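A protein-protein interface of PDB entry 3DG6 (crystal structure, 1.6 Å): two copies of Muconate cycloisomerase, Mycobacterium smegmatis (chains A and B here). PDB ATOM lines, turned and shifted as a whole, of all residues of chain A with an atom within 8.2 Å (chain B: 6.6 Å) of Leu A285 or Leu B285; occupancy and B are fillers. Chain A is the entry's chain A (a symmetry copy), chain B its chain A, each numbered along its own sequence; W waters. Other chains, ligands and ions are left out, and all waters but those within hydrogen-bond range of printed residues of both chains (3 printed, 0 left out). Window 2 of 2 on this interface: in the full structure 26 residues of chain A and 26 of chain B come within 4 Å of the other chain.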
ATOM      1  N   PRO A 248      -1.209 -27.178   9.121  1.00  0.00           N
ATOM      2  CA  PRO A 248      -1.208 -25.919   8.376  1.00  0.00           C
ATOM      3  C   PRO A 248      -0.401 -24.835   9.106  1.00  0.00           C
ATOM      4  O   PRO A 248       0.277 -24.027   8.476  1.00  0.00           O
ATOM      5  CB  PRO A 248      -2.694 -25.577   8.285  1.00  0.00           C
ATOM      6  CG  PRO A 248      -3.327 -26.940   8.173  1.00  0.00           C
ATOM      7  CD  PRO A 248      -2.575 -27.726   9.229  1.00  0.00           C
ATOM      8  N   ALA A 249      -0.470 -24.818  10.436  1.00  0.00           N
ATOM      9  CA  ALA A 249       0.271 -23.816  11.203  1.00  0.00           C
ATOM     10  C   ALA A 249       1.772 -23.984  10.980  1.00  0.00           C
ATOM     11  O   ALA A 249       2.513 -23.002  10.922  1.00  0.00           O
ATOM     12  CB  ALA A 249      -0.063 -23.932  12.690  1.00  0.00           C
ATOM     13  N   VAL A 251       3.078 -25.211   8.269  1.00  0.00           N
ATOM     14  CA  VAL A 251       3.327 -24.764   6.908  1.00  0.00           C
ATOM     15  C   VAL A 251       3.582 -23.259   6.938  1.00  0.00           C
ATOM     16  O   VAL A 251       4.553 -22.767   6.363  1.00  0.00           O
ATOM     17  CB  VAL A 251       2.122 -25.065   5.992  1.00  0.00           C
ATOM     18  CG1 VAL A 251       2.297 -24.381   4.638  1.00  0.00           C
ATOM     19  CG2 VAL A 251       1.987 -26.567   5.806  1.00  0.00           C
ATOM     20  N   THR A 252       2.714 -22.527   7.628  1.00  0.00           N
ATOM     21  CA  THR A 252       2.873 -21.084   7.710  1.00  0.00           C
ATOM     22  C   THR A 252       4.196 -20.681   8.361  1.00  0.00           C
ATOM     23  O   THR A 252       4.934 -19.864   7.811  1.00  0.00           O
ATOM     24  CB  THR A 252       1.687 -20.453   8.471  1.00  0.00           C
ATOM     25  OG1 THR A 252       0.488 -20.670   7.718  1.00  0.00           O
ATOM     26  CG2 THR A 252       1.896 -18.950   8.656  1.00  0.00           C
ATOM     27  N   ARG A 253       4.508 -21.257   9.519  1.00  0.00           N
ATOM     28  CA  ARG A 253       5.752 -20.917  10.208  1.00  0.00           C
ATOM     29  C   ARG A 253       7.006 -21.252   9.413  1.00  0.00           C
ATOM     30  O   ARG A 253       7.933 -20.443   9.339  1.00  0.00           O
ATOM     31  CB  ARG A 253       5.837 -21.621  11.566  1.00  0.00           C
ATOM     32  CG  ARG A 253       4.973 -21.005  12.655  1.00  0.00           C
ATOM     33  CD  ARG A 253       5.268 -21.668  13.998  1.00  0.00           C
ATOM     34  NE  ARG A 253       4.768 -23.040  14.053  1.00  0.00           N
ATOM     35  CZ  ARG A 253       3.569 -23.379  14.515  1.00  0.00           C
ATOM     36  NH1 ARG A 253       2.742 -22.450  14.972  1.00  0.00           N
ATOM     37  NH2 ARG A 253       3.188 -24.647  14.508  1.00  0.00           N
ATOM     38  N   GLU A 254       7.046 -22.442   8.823  1.00  0.00           N
ATOM     39  CA  GLU A 254       8.230 -22.843   8.069  1.00  0.00           C
ATOM     40  C   GLU A 254       8.384 -22.055   6.767  1.00  0.00           C
ATOM     41  O   GLU A 254       9.488 -21.670   6.397  1.00  0.00           O
ATOM     42  CB  GLU A 254       8.190 -24.345   7.768  1.00  0.00           C
ATOM     43  CG  GLU A 254       8.081 -25.253   9.007  1.00  0.00           C
ATOM     44  CD  GLU A 254       9.297 -25.209   9.926  1.00  0.00           C
ATOM     45  OE1 GLU A 254      10.442 -25.310   9.436  1.00  0.00           O
ATOM     46  OE2 GLU A 254       9.098 -25.100  11.154  1.00  0.00           O
ATOM     47  N   VAL A 255       7.282 -21.810   6.071  1.00  0.00           N
ATOM     48  CA  VAL A 255       7.366 -21.068   4.821  1.00  0.00           C
ATOM     49  C   VAL A 255       7.714 -19.597   5.039  1.00  0.00           C
ATOM     50  O   VAL A 255       8.598 -19.059   4.366  1.00  0.00           O
ATOM     51  CB  VAL A 255       6.056 -21.191   4.015  1.00  0.00           C
ATOM     52  CG1 VAL A 255       6.048 -20.197   2.866  1.00  0.00           C
ATOM     53  CG2 VAL A 255       5.933 -22.611   3.474  1.00  0.00           C
ATOM     54  N   LEU A 256       7.044 -18.945   5.984  1.00  0.00           N
ATOM     55  CA  LEU A 256       7.343 -17.539   6.230  1.00  0.00           C
ATOM     56  C   LEU A 256       8.726 -17.370   6.856  1.00  0.00           C
ATOM     57  O   LEU A 256       9.372 -16.337   6.672  1.00  0.00           O
ATOM     58  CB  LEU A 256       6.268 -16.907   7.122  1.00  0.00           C
ATOM     59  CG  LEU A 256       4.857 -16.896   6.525  1.00  0.00           C
ATOM     60  CD1 LEU A 256       3.912 -16.156   7.466  1.00  0.00           C
ATOM     61  CD2 LEU A 256       4.880 -16.229   5.151  1.00  0.00           C
ATOM     62  N   ILE A 263       5.835 -27.842  -0.342  1.00  0.00           N
ATOM     63  CA  ILE A 263       5.135 -28.605   0.686  1.00  0.00           C
ATOM     64  C   ILE A 263       4.696 -30.012   0.300  1.00  0.00           C
ATOM     65  O   ILE A 263       4.071 -30.215  -0.738  1.00  0.00           O
ATOM     66  CB  ILE A 263       3.870 -27.833   1.147  1.00  0.00           C
ATOM     67  CG1 ILE A 263       4.260 -26.442   1.661  1.00  0.00           C
ATOM     68  CG2 ILE A 263       3.118 -28.627   2.213  1.00  0.00           C
ATOM     69  CD1 ILE A 263       5.123 -26.458   2.905  1.00  0.00           C
ATOM     70  N   ARG A 277      -7.108 -28.231   3.633  1.00  0.00           N
ATOM     71  CA  ARG A 277      -6.624 -27.025   4.301  1.00  0.00           C
ATOM     72  C   ARG A 277      -5.177 -26.739   3.904  1.00  0.00           C
ATOM     73  O   ARG A 277      -4.802 -25.587   3.695  1.00  0.00           O
ATOM     74  CB  ARG A 277      -6.738 -27.167   5.822  1.00  0.00           C
ATOM     75  CG  ARG A 277      -8.147 -26.897   6.363  1.00  0.00           C
ATOM     76  CD  ARG A 277      -8.219 -27.161   7.856  1.00  0.00           C
ATOM     77  NE  ARG A 277      -9.310 -26.439   8.517  1.00  0.00           N
ATOM     78  CZ  ARG A 277     -10.602 -26.754   8.441  1.00  0.00           C
ATOM     79  NH1 ARG A 277     -11.010 -27.794   7.721  1.00  0.00           N
ATOM     80  NH2 ARG A 277     -11.489 -26.038   9.121  1.00  0.00           N
ATOM     81  N   VAL A 278      -4.363 -27.785   3.787  1.00  0.00           N
ATOM     82  CA  VAL A 278      -2.966 -27.605   3.402  1.00  0.00           C
ATOM     83  C   VAL A 278      -2.865 -27.173   1.935  1.00  0.00           C
ATOM     84  O   VAL A 278      -2.133 -26.237   1.601  1.00  0.00           O
ATOM     85  CB  VAL A 278      -2.153 -28.900   3.632  1.00  0.00           C
ATOM     86  CG1 VAL A 278      -0.719 -28.712   3.152  1.00  0.00           C
ATOM     87  CG2 VAL A 278      -2.159 -29.249   5.124  1.00  0.00           C
ATOM     88  N   HIS A 279      -3.606 -27.847   1.062  1.00  0.00           N
ATOM     89  CA  HIS A 279      -3.604 -27.498  -0.356  1.00  0.00           C
ATOM     90  C   HIS A 279      -4.006 -26.042  -0.566  1.00  0.00           C
ATOM     91  O   HIS A 279      -3.345 -25.300  -1.298  1.00  0.00           O
ATOM     92  CB  HIS A 279      -4.560 -28.413  -1.137  1.00  0.00           C
ATOM     93  CG  HIS A 279      -4.900 -27.908  -2.509  1.00  0.00           C
ATOM     94  ND1 HIS A 279      -5.787 -26.874  -2.724  1.00  0.00           N
ATOM     95  CD2 HIS A 279      -4.453 -28.278  -3.732  1.00  0.00           C
ATOM     96  CE1 HIS A 279      -5.871 -26.631  -4.020  1.00  0.00           C
ATOM     97  NE2 HIS A 279      -5.070 -27.470  -4.653  1.00  0.00           N
ATOM     98  N   HIS A 280      -5.090 -25.624   0.075  1.00  0.00           N
ATOM     99  CA  HIS A 280      -5.545 -24.254  -0.093  1.00  0.00           C
ATOM    100  C   HIS A 280      -4.566 -23.235   0.470  1.00  0.00           C
ATOM    101  O   HIS A 280      -4.398 -22.156  -0.100  1.00  0.00           O
ATOM    102  CB  HIS A 280      -6.942 -24.091   0.513  1.00  0.00           C
ATOM    103  CG  HIS A 280      -8.003 -24.795  -0.273  1.00  0.00           C
ATOM    104  ND1 HIS A 280      -9.350 -24.662  -0.011  1.00  0.00           N
ATOM    105  CD2 HIS A 280      -7.908 -25.640  -1.328  1.00  0.00           C
ATOM    106  CE1 HIS A 280     -10.038 -25.394  -0.871  1.00  0.00           C
ATOM    107  NE2 HIS A 280      -9.185 -25.998  -1.680  1.00  0.00           N
ATOM    108  N   LEU A 281      -3.909 -23.579   1.573  1.00  0.00           N
ATOM    109  CA  LEU A 281      -2.933 -22.671   2.163  1.00  0.00           C
ATOM    110  C   LEU A 281      -1.732 -22.554   1.221  1.00  0.00           C
ATOM    111  O   LEU A 281      -1.273 -21.452   0.919  1.00  0.00           O
ATOM    112  CB  LEU A 281      -2.480 -23.188   3.532  1.00  0.00           C
ATOM    113  CG  LEU A 281      -1.352 -22.417   4.227  1.00  0.00           C
ATOM    114  CD1 LEU A 281      -1.744 -20.958   4.437  1.00  0.00           C
ATOM    115  CD2 LEU A 281      -1.053 -23.084   5.562  1.00  0.00           C
ATOM    116  N   ALA A 282      -1.232 -23.694   0.749  1.00  0.00           N
ATOM    117  CA  ALA A 282      -0.088 -23.708  -0.160  1.00  0.00           C
ATOM    118  C   ALA A 282      -0.399 -23.011  -1.487  1.00  0.00           C
ATOM    119  O   ALA A 282       0.439 -22.285  -2.030  1.00  0.00           O
ATOM    120  CB  ALA A 282       0.360 -25.150  -0.411  1.00  0.00           C
ATOM    121  N   GLU A 283      -1.598 -23.230  -2.016  1.00  0.00           N
ATOM    122  CA  GLU A 283      -1.978 -22.596  -3.275  1.00  0.00           C
ATOM    123  C   GLU A 283      -2.091 -21.086  -3.071  1.00  0.00           C
ATOM    124  O   GLU A 283      -1.645 -20.300  -3.907  1.00  0.00           O
ATOM    125  CB  GLU A 283      -3.316 -23.148  -3.771  1.00  0.00           C
ATOM    126  CG  GLU A 283      -3.676 -22.714  -5.186  1.00  0.00           C
ATOM    127  CD  GLU A 283      -5.092 -23.106  -5.564  1.00  0.00           C
ATOM    128  OE1 GLU A 283      -6.031 -22.541  -4.974  1.00  0.00           O
ATOM    129  OE2 GLU A 283      -5.265 -23.981  -6.439  1.00  0.00           O
ATOM    130  N   GLY A 284      -2.679 -20.691  -1.946  1.00  0.00           N
ATOM    131  CA  GLY A 284      -2.848 -19.279  -1.649  1.00  0.00           C
ATOM    132  C   GLY A 284      -1.527 -18.568  -1.447  1.00  0.00           C
ATOM    133  O   GLY A 284      -1.359 -17.421  -1.865  1.00  0.00           O
ATOM    134  N   LEU A 285      -0.583 -19.241  -0.799  1.00  0.00           N
ATOM    135  CA  LEU A 285       0.730 -18.651  -0.565  1.00  0.00           C
ATOM    136  C   LEU A 285       1.558 -18.677  -1.839  1.00  0.00           C
ATOM    137  O   LEU A 285       2.455 -17.854  -2.012  1.00  0.00           O
ATOM    138  CB  LEU A 285       1.466 -19.398   0.549  1.00  0.00           C
ATOM    139  CG  LEU A 285       0.879 -19.153   1.941  1.00  0.00           C
ATOM    140  CD1 LEU A 285       1.659 -19.952   2.971  1.00  0.00           C
ATOM    141  CD2 LEU A 285       0.935 -17.661   2.267  1.00  0.00           C
ATOM    142  N   GLY A 286       1.248 -19.621  -2.725  1.00  0.00           N
ATOM    143  CA  GLY A 286       1.961 -19.735  -3.985  1.00  0.00           C
ATOM    144  C   GLY A 286       3.157 -20.664  -3.932  1.00  0.00           C
ATOM    145  O   GLY A 286       4.235 -20.315  -4.412  1.00  0.00           O
ATOM    146  N   LEU A 287       2.962 -21.850  -3.363  1.00  0.00           N
ATOM    147  CA  LEU A 287       4.030 -22.837  -3.225  1.00  0.00           C
ATOM    148  C   LEU A 287       3.683 -24.157  -3.892  1.00  0.00           C
ATOM    149  O   LEU A 287       2.519 -24.557  -3.915  1.00  0.00           O
ATOM    150  CB  LEU A 287       4.281 -23.120  -1.746  1.00  0.00           C
ATOM    151  CG  LEU A 287       4.560 -21.911  -0.859  1.00  0.00           C
ATOM    152  CD1 LEU A 287       4.418 -22.313   0.596  1.00  0.00           C
ATOM    153  CD2 LEU A 287       5.944 -21.368  -1.158  1.00  0.00           C
ATOM    154  N   ASP A 288       4.699 -24.836  -4.421  1.00  0.00           N
ATOM    155  CA  ASP A 288       4.483 -26.139  -5.039  1.00  0.00           C
ATOM    156  C   ASP A 288       4.154 -27.149  -3.953  1.00  0.00           C
ATOM    157  O   ASP A 288       4.600 -27.021  -2.811  1.00  0.00           O
ATOM    158  CB  ASP A 288       5.728 -26.622  -5.781  1.00  0.00           C
ATOM    159  CG  ASP A 288       5.930 -25.920  -7.098  1.00  0.00           C
ATOM    160  OD1 ASP A 288       4.963 -25.318  -7.605  1.00  0.00           O
ATOM    161  OD2 ASP A 288       7.055 -25.991  -7.632  1.00  0.00           O
ATOM    162  N   MET A 289       3.374 -28.159  -4.317  1.00  0.00           N
ATOM    163  CA  MET A 289       2.993 -29.202  -3.380  1.00  0.00           C
ATOM    164  C   MET A 289       3.047 -30.542  -4.095  1.00  0.00           C
ATOM    165  O   MET A 289       2.709 -30.639  -5.277  1.00  0.00           O
ATOM    166  CB  MET A 289       1.588 -28.930  -2.829  1.00  0.00           C
ATOM    167  CG  MET A 289       0.509 -28.808  -3.884  1.00  0.00           C
ATOM    168  SD  MET A 289      -1.001 -28.055  -3.232  1.00  0.00           S
ATOM    169  CE  MET A 289      -0.739 -26.330  -3.675  1.00  0.00           C
ATOM    170  N   PRO B 248      -7.727 -15.057  -3.343  1.00  0.00           N
ATOM    171  CA  PRO B 248      -6.768 -15.549  -2.355  1.00  0.00           C
ATOM    172  C   PRO B 248      -5.392 -14.890  -2.532  1.00  0.00           C
ATOM    173  O   PRO B 248      -4.702 -14.606  -1.555  1.00  0.00           O
ATOM    174  CB  PRO B 248      -6.735 -17.050  -2.632  1.00  0.00           C
ATOM    175  CG  PRO B 248      -8.158 -17.329  -3.041  1.00  0.00           C
ATOM    176  CD  PRO B 248      -8.449 -16.175  -3.980  1.00  0.00           C
ATOM    177  N   VAL B 251      -5.384 -11.730  -0.811  1.00  0.00           N
ATOM    178  CA  VAL B 251      -5.326 -11.932   0.628  1.00  0.00           C
ATOM    179  C   VAL B 251      -3.860 -12.064   1.034  1.00  0.00           C
ATOM    180  O   VAL B 251      -3.399 -11.413   1.971  1.00  0.00           O
ATOM    181  CB  VAL B 251      -6.093 -13.205   1.044  1.00  0.00           C
ATOM    182  CG1 VAL B 251      -5.823 -13.534   2.511  1.00  0.00           C
ATOM    183  CG2 VAL B 251      -7.581 -12.999   0.818  1.00  0.00           C
ATOM    184  N   THR B 252      -3.120 -12.897   0.312  1.00  0.00           N
ATOM    185  CA  THR B 252      -1.714 -13.090   0.626  1.00  0.00           C
ATOM    186  C   THR B 252      -0.909 -11.796   0.514  1.00  0.00           C
ATOM    187  O   THR B 252      -0.177 -11.439   1.436  1.00  0.00           O
ATOM    188  CB  THR B 252      -1.102 -14.181  -0.281  1.00  0.00           C
ATOM    189  OG1 THR B 252      -1.741 -15.430   0.006  1.00  0.00           O
ATOM    190  CG2 THR B 252       0.400 -14.318  -0.032  1.00  0.00           C
ATOM    191  N   VAL B 255      -2.110  -9.161   3.282  1.00  0.00           N
ATOM    192  CA  VAL B 255      -1.770  -9.566   4.640  1.00  0.00           C
ATOM    193  C   VAL B 255      -0.265  -9.556   4.891  1.00  0.00           C
ATOM    194  O   VAL B 255       0.195  -9.022   5.905  1.00  0.00           O
ATOM    195  CB  VAL B 255      -2.356 -10.955   4.965  1.00  0.00           C
ATOM    196  CG1 VAL B 255      -1.767 -11.486   6.261  1.00  0.00           C
ATOM    197  CG2 VAL B 255      -3.871 -10.843   5.091  1.00  0.00           C
ATOM    198  N   LEU B 256       0.511 -10.124   3.973  1.00  0.00           N
ATOM    199  CA  LEU B 256       1.956 -10.137   4.169  1.00  0.00           C
ATOM    200  C   LEU B 256       2.544  -8.733   4.042  1.00  0.00           C
ATOM    201  O   LEU B 256       3.572  -8.430   4.650  1.00  0.00           O
ATOM    202  CB  LEU B 256       2.627 -11.092   3.175  1.00  0.00           C
ATOM    203  CG  LEU B 256       2.212 -12.561   3.309  1.00  0.00           C
ATOM    204  CD1 LEU B 256       3.020 -13.410   2.333  1.00  0.00           C
ATOM    205  CD2 LEU B 256       2.432 -13.034   4.744  1.00  0.00           C
ATOM    206  N   HIS B 280      -9.644 -21.239   4.233  1.00  0.00           N
ATOM    207  CA  HIS B 280      -8.488 -22.049   4.579  1.00  0.00           C
ATOM    208  C   HIS B 280      -7.193 -21.253   4.592  1.00  0.00           C
ATOM    209  O   HIS B 280      -6.321 -21.502   5.426  1.00  0.00           O
ATOM    210  CB  HIS B 280      -8.401 -23.257   3.641  1.00  0.00           C
ATOM    211  CG  HIS B 280      -9.481 -24.263   3.885  1.00  0.00           C
ATOM    212  ND1 HIS B 280      -9.514 -25.498   3.273  1.00  0.00           N
ATOM    213  CD2 HIS B 280     -10.571 -24.213   4.687  1.00  0.00           C
ATOM    214  CE1 HIS B 280     -10.579 -26.164   3.690  1.00  0.00           C
ATOM    215  NE2 HIS B 280     -11.237 -25.405   4.547  1.00  0.00           N
ATOM    216  N   LEU B 281      -7.072 -20.288   3.687  1.00  0.00           N
ATOM    217  CA  LEU B 281      -5.873 -19.459   3.648  1.00  0.00           C
ATOM    218  C   LEU B 281      -5.833 -18.586   4.904  1.00  0.00           C
ATOM    219  O   LEU B 281      -4.808 -18.504   5.582  1.00  0.00           O
ATOM    220  CB  LEU B 281      -5.871 -18.579   2.394  1.00  0.00           C
ATOM    221  CG  LEU B 281      -4.742 -17.549   2.271  1.00  0.00           C
ATOM    222  CD1 LEU B 281      -3.380 -18.232   2.307  1.00  0.00           C
ATOM    223  CD2 LEU B 281      -4.919 -16.783   0.967  1.00  0.00           C
ATOM    224  N   ALA B 282      -6.956 -17.943   5.218  1.00  0.00           N
ATOM    225  CA  ALA B 282      -7.039 -17.082   6.396  1.00  0.00           C
ATOM    226  C   ALA B 282      -6.835 -17.865   7.696  1.00  0.00           C
ATOM    227  O   ALA B 282      -6.168 -17.389   8.620  1.00  0.00           O
ATOM    228  CB  ALA B 282      -8.388 -16.359   6.419  1.00  0.00           C
ATOM    229  N   GLU B 283      -7.408 -19.060   7.776  1.00  0.00           N
ATOM    230  CA  GLU B 283      -7.255 -19.875   8.978  1.00  0.00           C
ATOM    231  C   GLU B 283      -5.797 -20.312   9.115  1.00  0.00           C
ATOM    232  O   GLU B 283      -5.231 -20.289  10.207  1.00  0.00           O
ATOM    233  CB  GLU B 283      -8.155 -21.110   8.907  1.00  0.00           C
ATOM    234  CG  GLU B 283      -8.233 -21.894  10.210  1.00  0.00           C
ATOM    235  CD  GLU B 283      -8.961 -23.213  10.045  1.00  0.00           C
ATOM    236  OE1 GLU B 283      -8.421 -24.096   9.354  1.00  0.00           O
ATOM    237  OE2 GLU B 283     -10.074 -23.364  10.595  1.00  0.00           O
ATOM    238  N   GLY B 284      -5.195 -20.695   7.993  1.00  0.00           N
ATOM    239  CA  GLY B 284      -3.811 -21.137   8.004  1.00  0.00           C
ATOM    240  C   GLY B 284      -2.851 -20.028   8.380  1.00  0.00           C
ATOM    241  O   GLY B 284      -1.870 -20.258   9.089  1.00  0.00           O
ATOM    242  N   LEU B 285      -3.124 -18.819   7.902  1.00  0.00           N
ATOM    243  CA  LEU B 285      -2.271 -17.679   8.217  1.00  0.00           C
ATOM    244  C   LEU B 285      -2.529 -17.199   9.635  1.00  0.00           C
ATOM    245  O   LEU B 285      -1.651 -16.605  10.258  1.00  0.00           O
ATOM    246  CB  LEU B 285      -2.511 -16.537   7.229  1.00  0.00           C
ATOM    247  CG  LEU B 285      -1.970 -16.817   5.825  1.00  0.00           C
ATOM    248  CD1 LEU B 285      -2.276 -15.640   4.915  1.00  0.00           C
ATOM    249  CD2 LEU B 285      -0.463 -17.063   5.895  1.00  0.00           C
ATOM    250  N   GLY B 286      -3.734 -17.463  10.137  1.00  0.00           N
ATOM    251  CA  GLY B 286      -4.091 -17.065  11.487  1.00  0.00           C
ATOM    252  C   GLY B 286      -4.737 -15.697  11.574  1.00  0.00           C
ATOM    253  O   GLY B 286      -4.363 -14.888  12.422  1.00  0.00           O
ATOM    254  N   LEU B 287      -5.715 -15.448  10.708  1.00  0.00           N
ATOM    255  CA  LEU B 287      -6.412 -14.165  10.664  1.00  0.00           C
ATOM    256  C   LEU B 287      -7.910 -14.318  10.863  1.00  0.00           C
ATOM    257  O   LEU B 287      -8.497 -15.316  10.442  1.00  0.00           O
ATOM    258  CB  LEU B 287      -6.193 -13.507   9.303  1.00  0.00           C
ATOM    259  CG  LEU B 287      -4.746 -13.338   8.855  1.00  0.00           C
ATOM    260  CD1 LEU B 287      -4.714 -13.024   7.371  1.00  0.00           C
ATOM    261  CD2 LEU B 287      -4.083 -12.246   9.672  1.00  0.00           C
HETATM  262  O   HOH W   1      -7.941 -26.476  11.691  1.00  0.00           O
HETATM  263  O   HOH W   2      -5.106 -23.893   5.999  1.00  0.00           O
HETATM  264  O   HOH W   3     -11.103 -28.778   4.518  1.00  0.00           O
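Hydrophobic or aromatic side chains of chain B within 4 Å of the printed part of chain A: His B280, Leu B281 and Leu B285.
Of the 22 printed residues of chain A, 6 touch a printed residue of chain B.
Hydrophobic or aromatic side chains of chain A within 4 Å of the printed part of chain B: His A280, Leu A281 and Leu A285.
Among the printed residues, 7 pairs touch across the chains.
Of chain A, only Leu A285 (3.9 Å) comes within 4 Å of Leu B285.
Gly B284 touches just one residue of chain A: Thr A252 (2.8 Å).
Of the printed residues of chain A, Glu B283 touches Arg A277 (2.6 Å).
Printed residues of chain B within 4 Å of Leu A281: Leu B281.
Of the printed residues of chain A, His B280 touches Arg A277 and His A280.
Of the printed residues of chain B, His A280 touches His B280 (3.4 Å).
Printed residues of chain A within 4 Å of Thr B252: Gly A284 (2.8 Å).
The nearest residue of chain B that does not touch Leu A285 is Thr B252 (4.1 Å).
The nearest residue of chain A that does not touch Leu B285 is Thr A252 (4.1 Å).
The nearest printed residue of chain B that does not touch Leu A281 is Gly B284 (4.1 Å).
Water W2 lies within hydrogen-bond range of O of His B280 and O of Arg A277.
Water W3 bridges the guanidinium group (NH1) of Arg A277 (3.4 Å) and a ring nitrogen (NE2) of His B280 (3.4 Å).
Water W1 bridges the side-chain carboxylate (OE1) of Glu B283 (3.4 Å) and the guanidinium group (NE) of Arg A277 (3.5 Å).
Among the printed residues, merely in contact across the chains: Arg A277 with His B280, Leu A281 with Leu B281 and Leu A285 with Leu B285.
OG1 of Thr B252 sits at hydrogen-bond distance from O of Gly A284 (2.8 Å).
A ring nitrogen (ND1) of His B280 lies within hydrogen-bond range of a ring nitrogen (ND1) of His A280, 3.4 Å away.
NE of Arg A277 lies within salt-bridge range of OE1 of Glu B283 (2.6 Å).
The backbone carbonyl oxygen (O) of Gly B284 is in hydrogen-bond range of the side-chain hydroxyl (OG1) of Thr A252, 2.8 Å away.
O of Pro B248 lies within hydrogen-bond range of OG1 of Thr B252 (3.4 Å).
The side-chain hydroxyl (OG1) of Thr A252 lies within hydrogen-bond range of the backbone carbonyl oxygen (O) of Pro A248.
Thr A252 touches Gly B284, and with the chains exchanged Gly A284 touches Thr B252.
His B280 touches its own counterpart, His A280.
Leu A281 touches its own counterpart, Leu B281.
Leu A285 touches its own counterpart, Leu B285.
Of the 7 pairs that touch across the chains among the printed residues, 5 have their exchanged pair printed and touching as well.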
